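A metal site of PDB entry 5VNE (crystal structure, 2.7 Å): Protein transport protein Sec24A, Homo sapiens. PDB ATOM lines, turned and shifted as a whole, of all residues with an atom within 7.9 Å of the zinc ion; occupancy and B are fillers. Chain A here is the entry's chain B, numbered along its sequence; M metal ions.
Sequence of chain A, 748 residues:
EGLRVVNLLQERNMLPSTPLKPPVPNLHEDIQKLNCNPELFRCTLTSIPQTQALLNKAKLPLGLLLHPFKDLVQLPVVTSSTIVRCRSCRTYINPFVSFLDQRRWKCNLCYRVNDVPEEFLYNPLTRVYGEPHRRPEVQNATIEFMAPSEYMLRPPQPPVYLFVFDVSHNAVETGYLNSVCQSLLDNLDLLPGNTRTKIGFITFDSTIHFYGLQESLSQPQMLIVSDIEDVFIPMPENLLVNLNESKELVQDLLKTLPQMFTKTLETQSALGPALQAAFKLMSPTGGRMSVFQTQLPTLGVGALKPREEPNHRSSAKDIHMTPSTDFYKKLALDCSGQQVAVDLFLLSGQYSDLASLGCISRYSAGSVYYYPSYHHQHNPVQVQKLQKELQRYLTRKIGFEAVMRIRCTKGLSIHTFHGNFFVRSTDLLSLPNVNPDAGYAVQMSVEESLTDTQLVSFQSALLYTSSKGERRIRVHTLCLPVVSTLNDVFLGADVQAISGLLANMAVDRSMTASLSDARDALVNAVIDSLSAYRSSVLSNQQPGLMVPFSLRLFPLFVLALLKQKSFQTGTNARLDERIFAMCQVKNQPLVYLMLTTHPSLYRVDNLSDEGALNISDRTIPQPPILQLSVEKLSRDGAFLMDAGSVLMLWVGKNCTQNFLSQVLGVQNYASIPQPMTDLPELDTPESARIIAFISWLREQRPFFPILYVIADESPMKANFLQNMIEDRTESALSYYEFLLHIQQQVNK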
ATOM      1  N   ARG A  85     -24.237 -28.307  19.583  1.00  0.00           N
ATOM      2  CA  ARG A  85     -23.765 -28.895  20.823  1.00  0.00           C
ATOM      3  C   ARG A  85     -22.346 -29.408  20.632  1.00  0.00           C
ATOM      4  O   ARG A  85     -21.973 -29.840  19.544  1.00  0.00           O
ATOM      5  CB  ARG A  85     -24.678 -30.034  21.287  1.00  0.00           C
ATOM      6  CG  ARG A  85     -26.097 -29.600  21.622  1.00  0.00           C
ATOM      7  CD  ARG A  85     -27.025 -30.768  21.882  1.00  0.00           C
ATOM      8  NE  ARG A  85     -26.869 -31.321  23.227  1.00  0.00           N
ATOM      9  CZ  ARG A  85     -27.805 -32.022  23.859  1.00  0.00           C
ATOM     10  NH1 ARG A  85     -27.584 -32.490  25.078  1.00  0.00           N
ATOM     11  NH2 ARG A  85     -28.962 -32.248  23.263  1.00  0.00           N
ATOM     12  N   CYS A  86     -21.557 -29.326  21.703  1.00  0.00           N
ATOM     13  CA  CYS A  86     -20.222 -29.892  21.684  1.00  0.00           C
ATOM     14  C   CYS A  86     -20.300 -31.398  21.473  1.00  0.00           C
ATOM     15  O   CYS A  86     -20.940 -32.113  22.252  1.00  0.00           O
ATOM     16  CB  CYS A  86     -19.493 -29.570  22.996  1.00  0.00           C
ATOM     17  SG  CYS A  86     -17.803 -30.190  23.073  1.00  0.00           S
ATOM     18  N   ARG A  87     -19.656 -31.881  20.401  1.00  0.00           N
ATOM     19  CA  ARG A  87     -19.852 -33.257  19.970  1.00  0.00           C
ATOM     20  C   ARG A  87     -19.391 -34.273  21.012  1.00  0.00           C
ATOM     21  O   ARG A  87     -19.780 -35.444  20.930  1.00  0.00           O
ATOM     22  CB  ARG A  87     -19.130 -33.505  18.652  1.00  0.00           C
ATOM     23  CG  ARG A  87     -19.579 -34.765  17.923  1.00  0.00           C
ATOM     24  CD  ARG A  87     -18.566 -35.192  16.871  1.00  0.00           C
ATOM     25  NE  ARG A  87     -19.043 -34.923  15.508  1.00  0.00           N
ATOM     26  CZ  ARG A  87     -18.354 -35.220  14.419  1.00  0.00           C
ATOM     27  NH1 ARG A  87     -18.843 -34.936  13.223  1.00  0.00           N
ATOM     28  NH2 ARG A  87     -17.154 -35.792  14.521  1.00  0.00           N
ATOM     29  N   SER A  88     -18.589 -33.868  21.989  1.00  0.00           N
ATOM     30  CA  SER A  88     -18.064 -34.809  22.977  1.00  0.00           C
ATOM     31  C   SER A  88     -18.854 -34.853  24.268  1.00  0.00           C
ATOM     32  O   SER A  88     -18.969 -35.927  24.878  1.00  0.00           O
ATOM     33  CB  SER A  88     -16.598 -34.480  23.293  1.00  0.00           C
ATOM     34  OG  SER A  88     -15.861 -35.659  23.557  1.00  0.00           O
ATOM     35  N   CYS A  89     -19.415 -33.720  24.728  1.00  0.00           N
ATOM     36  CA  CYS A  89     -20.182 -33.684  25.956  1.00  0.00           C
ATOM     37  C   CYS A  89     -21.585 -33.109  25.793  1.00  0.00           C
ATOM     38  O   CYS A  89     -22.322 -33.044  26.787  1.00  0.00           O
ATOM     39  CB  CYS A  89     -19.439 -32.880  27.035  1.00  0.00           C
ATOM     40  SG  CYS A  89     -19.572 -31.090  26.858  1.00  0.00           S
ATOM     41  N   ARG A  90     -21.962 -32.683  24.591  1.00  0.00           N
ATOM     42  CA  ARG A  90     -23.317 -32.228  24.257  1.00  0.00           C
ATOM     43  C   ARG A  90     -23.732 -30.974  25.022  1.00  0.00           C
ATOM     44  O   ARG A  90     -24.925 -30.721  25.196  1.00  0.00           O
ATOM     45  CB  ARG A  90     -24.344 -33.339  24.488  1.00  0.00           C
ATOM     46  CG  ARG A  90     -24.166 -34.537  23.588  1.00  0.00           C
ATOM     47  CD  ARG A  90     -24.769 -35.769  24.234  1.00  0.00           C
ATOM     48  NE  ARG A  90     -25.357 -36.677  23.262  1.00  0.00           N
ATOM     49  CZ  ARG A  90     -26.049 -37.760  23.583  1.00  0.00           C
ATOM     50  NH1 ARG A  90     -26.245 -38.060  24.858  1.00  0.00           N
ATOM     51  NH2 ARG A  90     -26.563 -38.534  22.640  1.00  0.00           N
ATOM     52  N   THR A  91     -22.769 -30.176  25.472  1.00  0.00           N
ATOM     53  CA  THR A  91     -23.102 -28.890  26.073  1.00  0.00           C
ATOM     54  C   THR A  91     -23.659 -27.955  25.012  1.00  0.00           C
ATOM     55  O   THR A  91     -23.090 -27.814  23.926  1.00  0.00           O
ATOM     56  CB  THR A  91     -21.867 -28.265  26.728  1.00  0.00           C
ATOM     57  OG1 THR A  91     -21.370 -29.137  27.740  1.00  0.00           O
ATOM     58  CG2 THR A  91     -22.210 -26.920  27.344  1.00  0.00           C
ATOM     59  N   TYR A  92     -24.790 -27.327  25.306  1.00  0.00           N
ATOM     60  CA  TYR A  92     -25.416 -26.420  24.356  1.00  0.00           C
ATOM     61  C   TYR A  92     -24.552 -25.185  24.148  1.00  0.00           C
ATOM     62  O   TYR A  92     -23.802 -24.761  25.033  1.00  0.00           O
ATOM     63  CB  TYR A  92     -26.813 -26.004  24.853  1.00  0.00           C
ATOM     64  CG  TYR A  92     -27.802 -27.148  24.957  1.00  0.00           C
ATOM     65  CD1 TYR A  92     -27.712 -28.091  25.977  1.00  0.00           C
ATOM     66  CD2 TYR A  92     -28.823 -27.285  24.031  1.00  0.00           C
ATOM     67  CE1 TYR A  92     -28.616 -29.125  26.072  1.00  0.00           C
ATOM     68  CE2 TYR A  92     -29.738 -28.325  24.121  1.00  0.00           C
ATOM     69  CZ  TYR A  92     -29.625 -29.243  25.137  1.00  0.00           C
ATOM     70  OH  TYR A  92     -30.528 -30.277  25.232  1.00  0.00           O
ATOM     71  N   ASN A  94     -23.504 -21.516  24.146  1.00  0.00           N
ATOM     72  CA  ASN A  94     -23.806 -20.600  25.236  1.00  0.00           C
ATOM     73  C   ASN A  94     -22.973 -19.338  25.068  1.00  0.00           C
ATOM     74  O   ASN A  94     -21.994 -19.334  24.314  1.00  0.00           O
ATOM     75  CB  ASN A  94     -23.529 -21.249  26.600  1.00  0.00           C
ATOM     76  CG  ASN A  94     -22.095 -21.730  26.743  1.00  0.00           C
ATOM     77  OD1 ASN A  94     -21.295 -21.134  27.459  1.00  0.00           O
ATOM     78  ND2 ASN A  94     -21.767 -22.832  26.068  1.00  0.00           N
ATOM     79  N   TRP A 105     -15.868 -23.080  17.378  1.00  0.00           N
ATOM     80  CA  TRP A 105     -16.119 -22.569  18.718  1.00  0.00           C
ATOM     81  C   TRP A 105     -15.525 -23.511  19.759  1.00  0.00           C
ATOM     82  O   TRP A 105     -15.429 -24.726  19.545  1.00  0.00           O
ATOM     83  CB  TRP A 105     -17.613 -22.371  18.984  1.00  0.00           C
ATOM     84  CG  TRP A 105     -18.489 -23.572  18.756  1.00  0.00           C
ATOM     85  CD1 TRP A 105     -18.900 -24.077  17.555  1.00  0.00           C
ATOM     86  CD2 TRP A 105     -19.089 -24.398  19.759  1.00  0.00           C
ATOM     87  NE1 TRP A 105     -19.706 -25.178  17.751  1.00  0.00           N
ATOM     88  CE2 TRP A 105     -19.838 -25.398  19.100  1.00  0.00           C
ATOM     89  CE3 TRP A 105     -19.059 -24.403  21.158  1.00  0.00           C
ATOM     90  CZ2 TRP A 105     -20.542 -26.380  19.779  1.00  0.00           C
ATOM     91  CZ3 TRP A 105     -19.771 -25.369  21.838  1.00  0.00           C
ATOM     92  CH2 TRP A 105     -20.500 -26.352  21.154  1.00  0.00           C
ATOM     93  N   LYS A 106     -15.134 -22.934  20.890  1.00  0.00           N
ATOM     94  CA  LYS A 106     -14.412 -23.643  21.943  1.00  0.00           C
ATOM     95  C   LYS A 106     -15.340 -23.779  23.150  1.00  0.00           C
ATOM     96  O   LYS A 106     -15.417 -22.884  23.997  1.00  0.00           O
ATOM     97  CB  LYS A 106     -13.113 -22.903  22.306  1.00  0.00           C
ATOM     98  CG  LYS A 106     -11.937 -23.795  22.698  1.00  0.00           C
ATOM     99  CD  LYS A 106     -12.255 -25.278  22.567  1.00  0.00           C
ATOM    100  CE  LYS A 106     -12.676 -25.851  23.903  1.00  0.00           C
ATOM    101  NZ  LYS A 106     -13.890 -26.700  23.793  1.00  0.00           N
ATOM    102  N   CYS A 107     -16.038 -24.921  23.223  1.00  0.00           N
ATOM    103  CA  CYS A 107     -16.943 -25.201  24.321  1.00  0.00           C
ATOM    104  C   CYS A 107     -16.263 -24.970  25.671  1.00  0.00           C
ATOM    105  O   CYS A 107     -15.114 -25.373  25.878  1.00  0.00           O
ATOM    106  CB  CYS A 107     -17.443 -26.642  24.232  1.00  0.00           C
ATOM    107  SG  CYS A 107     -18.380 -27.217  25.670  1.00  0.00           S
ATOM    108  N   ASN A 108     -16.989 -24.324  26.581  1.00  0.00           N
ATOM    109  CA  ASN A 108     -16.455 -23.904  27.864  1.00  0.00           C
ATOM    110  C   ASN A 108     -16.615 -24.959  28.961  1.00  0.00           C
ATOM    111  O   ASN A 108     -16.496 -24.621  30.146  1.00  0.00           O
ATOM    112  CB  ASN A 108     -17.118 -22.601  28.294  1.00  0.00           C
ATOM    113  CG  ASN A 108     -18.627 -22.644  28.166  1.00  0.00           C
ATOM    114  OD1 ASN A 108     -19.166 -23.353  27.325  1.00  0.00           O
ATOM    115  ND2 ASN A 108     -19.317 -21.885  29.004  1.00  0.00           N
ATOM    116  N   LEU A 109     -16.865 -26.211  28.593  1.00  0.00           N
ATOM    117  CA  LEU A 109     -17.126 -27.241  29.605  1.00  0.00           C
ATOM    118  C   LEU A 109     -16.189 -28.434  29.524  1.00  0.00           C
ATOM    119  O   LEU A 109     -15.810 -28.973  30.577  1.00  0.00           O
ATOM    120  CB  LEU A 109     -18.581 -27.727  29.512  1.00  0.00           C
ATOM    121  CG  LEU A 109     -19.570 -27.008  30.441  1.00  0.00           C
ATOM    122  CD1 LEU A 109     -19.919 -25.623  29.911  1.00  0.00           C
ATOM    123  CD2 LEU A 109     -20.825 -27.839  30.652  1.00  0.00           C
ATOM    124  N   CYS A 110     -15.803 -28.886  28.334  1.00  0.00           N
ATOM    125  CA  CYS A 110     -14.974 -30.079  28.212  1.00  0.00           C
ATOM    126  C   CYS A 110     -13.698 -29.869  27.401  1.00  0.00           C
ATOM    127  O   CYS A 110     -12.919 -30.820  27.261  1.00  0.00           O
ATOM    128  CB  CYS A 110     -15.779 -31.234  27.600  1.00  0.00           C
ATOM    129  SG  CYS A 110     -15.997 -31.132  25.814  1.00  0.00           S
ATOM    130  N   TYR A 111     -13.489 -28.678  26.831  1.00  0.00           N
ATOM    131  CA  TYR A 111     -12.228 -28.323  26.184  1.00  0.00           C
ATOM    132  C   TYR A 111     -11.959 -29.182  24.955  1.00  0.00           C
ATOM    133  O   TYR A 111     -10.836 -29.635  24.716  1.00  0.00           O
ATOM    134  CB  TYR A 111     -11.069 -28.366  27.184  1.00  0.00           C
ATOM    135  CG  TYR A 111     -11.338 -27.459  28.362  1.00  0.00           C
ATOM    136  CD1 TYR A 111     -11.942 -26.225  28.176  1.00  0.00           C
ATOM    137  CD2 TYR A 111     -11.022 -27.845  29.658  1.00  0.00           C
ATOM    138  CE1 TYR A 111     -12.219 -25.393  29.242  1.00  0.00           C
ATOM    139  CE2 TYR A 111     -11.287 -27.014  30.737  1.00  0.00           C
ATOM    140  CZ  TYR A 111     -11.888 -25.788  30.514  1.00  0.00           C
ATOM    141  OH  TYR A 111     -12.165 -24.942  31.566  1.00  0.00           O
ATOM    142  N   ARG A 112     -13.004 -29.410  24.163  1.00  0.00           N
ATOM    143  CA  ARG A 112     -12.917 -30.012  22.836  1.00  0.00           C
ATOM    144  C   ARG A 112     -13.427 -29.003  21.816  1.00  0.00           C
ATOM    145  O   ARG A 112     -14.514 -28.443  21.990  1.00  0.00           O
ATOM    146  CB  ARG A 112     -13.721 -31.317  22.771  1.00  0.00           C
ATOM    147  CG  ARG A 112     -14.423 -31.565  21.432  1.00  0.00           C
ATOM    148  CD  ARG A 112     -13.552 -32.369  20.481  1.00  0.00           C
ATOM    149  NE  ARG A 112     -14.226 -33.606  20.065  1.00  0.00           N
ATOM    150  CZ  ARG A 112     -14.980 -33.722  18.989  1.00  0.00           C
ATOM    151  NH1 ARG A 112     -15.554 -34.890  18.693  1.00  0.00           N
ATOM    152  NH2 ARG A 112     -15.174 -32.677  18.192  1.00  0.00           N
ATOM    153  N   VAL A 113     -12.641 -28.755  20.773  1.00  0.00           N
ATOM    154  CA  VAL A 113     -12.991 -27.738  19.785  1.00  0.00           C
ATOM    155  C   VAL A 113     -14.013 -28.320  18.810  1.00  0.00           C
ATOM    156  O   VAL A 113     -13.845 -29.429  18.296  1.00  0.00           O
ATOM    157  CB  VAL A 113     -11.731 -27.236  19.057  1.00  0.00           C
ATOM    158  CG1 VAL A 113     -10.899 -28.396  18.526  1.00  0.00           C
ATOM    159  CG2 VAL A 113     -12.115 -26.292  17.918  1.00  0.00           C
ATOM    160  N   ASN A 114     -15.085 -27.565  18.563  1.00  0.00           N
ATOM    161  CA  ASN A 114     -16.151 -27.974  17.670  1.00  0.00           C
ATOM    162  C   ASN A 114     -16.278 -27.002  16.513  1.00  0.00           C
ATOM    163  O   ASN A 114     -15.816 -25.857  16.570  1.00  0.00           O
ATOM    164  CB  ASN A 114     -17.492 -28.077  18.418  1.00  0.00           C
ATOM    165  CG  ASN A 114     -17.634 -29.369  19.195  1.00  0.00           C
ATOM    166  OD1 ASN A 114     -18.448 -30.227  18.836  1.00  0.00           O
ATOM    167  ND2 ASN A 114     -16.833 -29.525  20.232  1.00  0.00           N
ATOM    168  N   ARG A 407     -24.856 -29.880  33.709  1.00  0.00           N
ATOM    169  CA  ARG A 407     -23.476 -30.076  33.297  1.00  0.00           C
ATOM    170  C   ARG A 407     -22.606 -28.961  33.842  1.00  0.00           C
ATOM    171  O   ARG A 407     -23.040 -27.809  33.975  1.00  0.00           O
ATOM    172  CB  ARG A 407     -23.359 -30.118  31.769  1.00  0.00           C
ATOM    173  CG  ARG A 407     -24.060 -31.283  31.106  1.00  0.00           C
ATOM    174  CD  ARG A 407     -23.892 -31.203  29.596  1.00  0.00           C
ATOM    175  NE  ARG A 407     -24.472 -32.357  28.914  1.00  0.00           N
ATOM    176  CZ  ARG A 407     -25.732 -32.419  28.489  1.00  0.00           C
ATOM    177  NH1 ARG A 407     -26.554 -31.402  28.691  1.00  0.00           N
ATOM    178  NH2 ARG A 407     -26.170 -33.504  27.868  1.00  0.00           N
HETATM  179 ZN    ZN M   1     -18.075 -29.761  25.491  1.00  0.00          ZN
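SG of Cys 89 lies close to OG1 of Thr 91 (2.8 Å).
The backbone carbonyl oxygen (O) of Cys 89 is in hydrogen-bond range of the guanidinium group (NE) of Arg 407 (3.1 Å).
The backbone carbonyl oxygen (O) of Thr 91 is in hydrogen-bond range of the backbone NH (N) of Cys 86 (3.1 Å).
ND2 of Asn 114 lies close to SG of Cys 86 (3.1 Å).
The side-chain sulfur (SG) of Cys 107 sits close to the backbone NH (N) of Leu 109, 3.4 Å away.
The zinc ion is bound by the side-chain sulfur of Cys 89 (2.4 Å), the side-chain sulfur of Cys 86 (2.5 Å), the side-chain sulfur of Cys 110 (2.5 Å) and the side-chain sulfur of Cys 107 (2.6 Å).
The zinc ion has four donor atoms within binding distance.
Four residues have an atom within 4 Å of the zinc ion: Cys 86, Cys 89, Cys 107 and Cys 110.
The nearest printed residue that does not touch the zinc ion is Thr 91 (4.04 Å).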
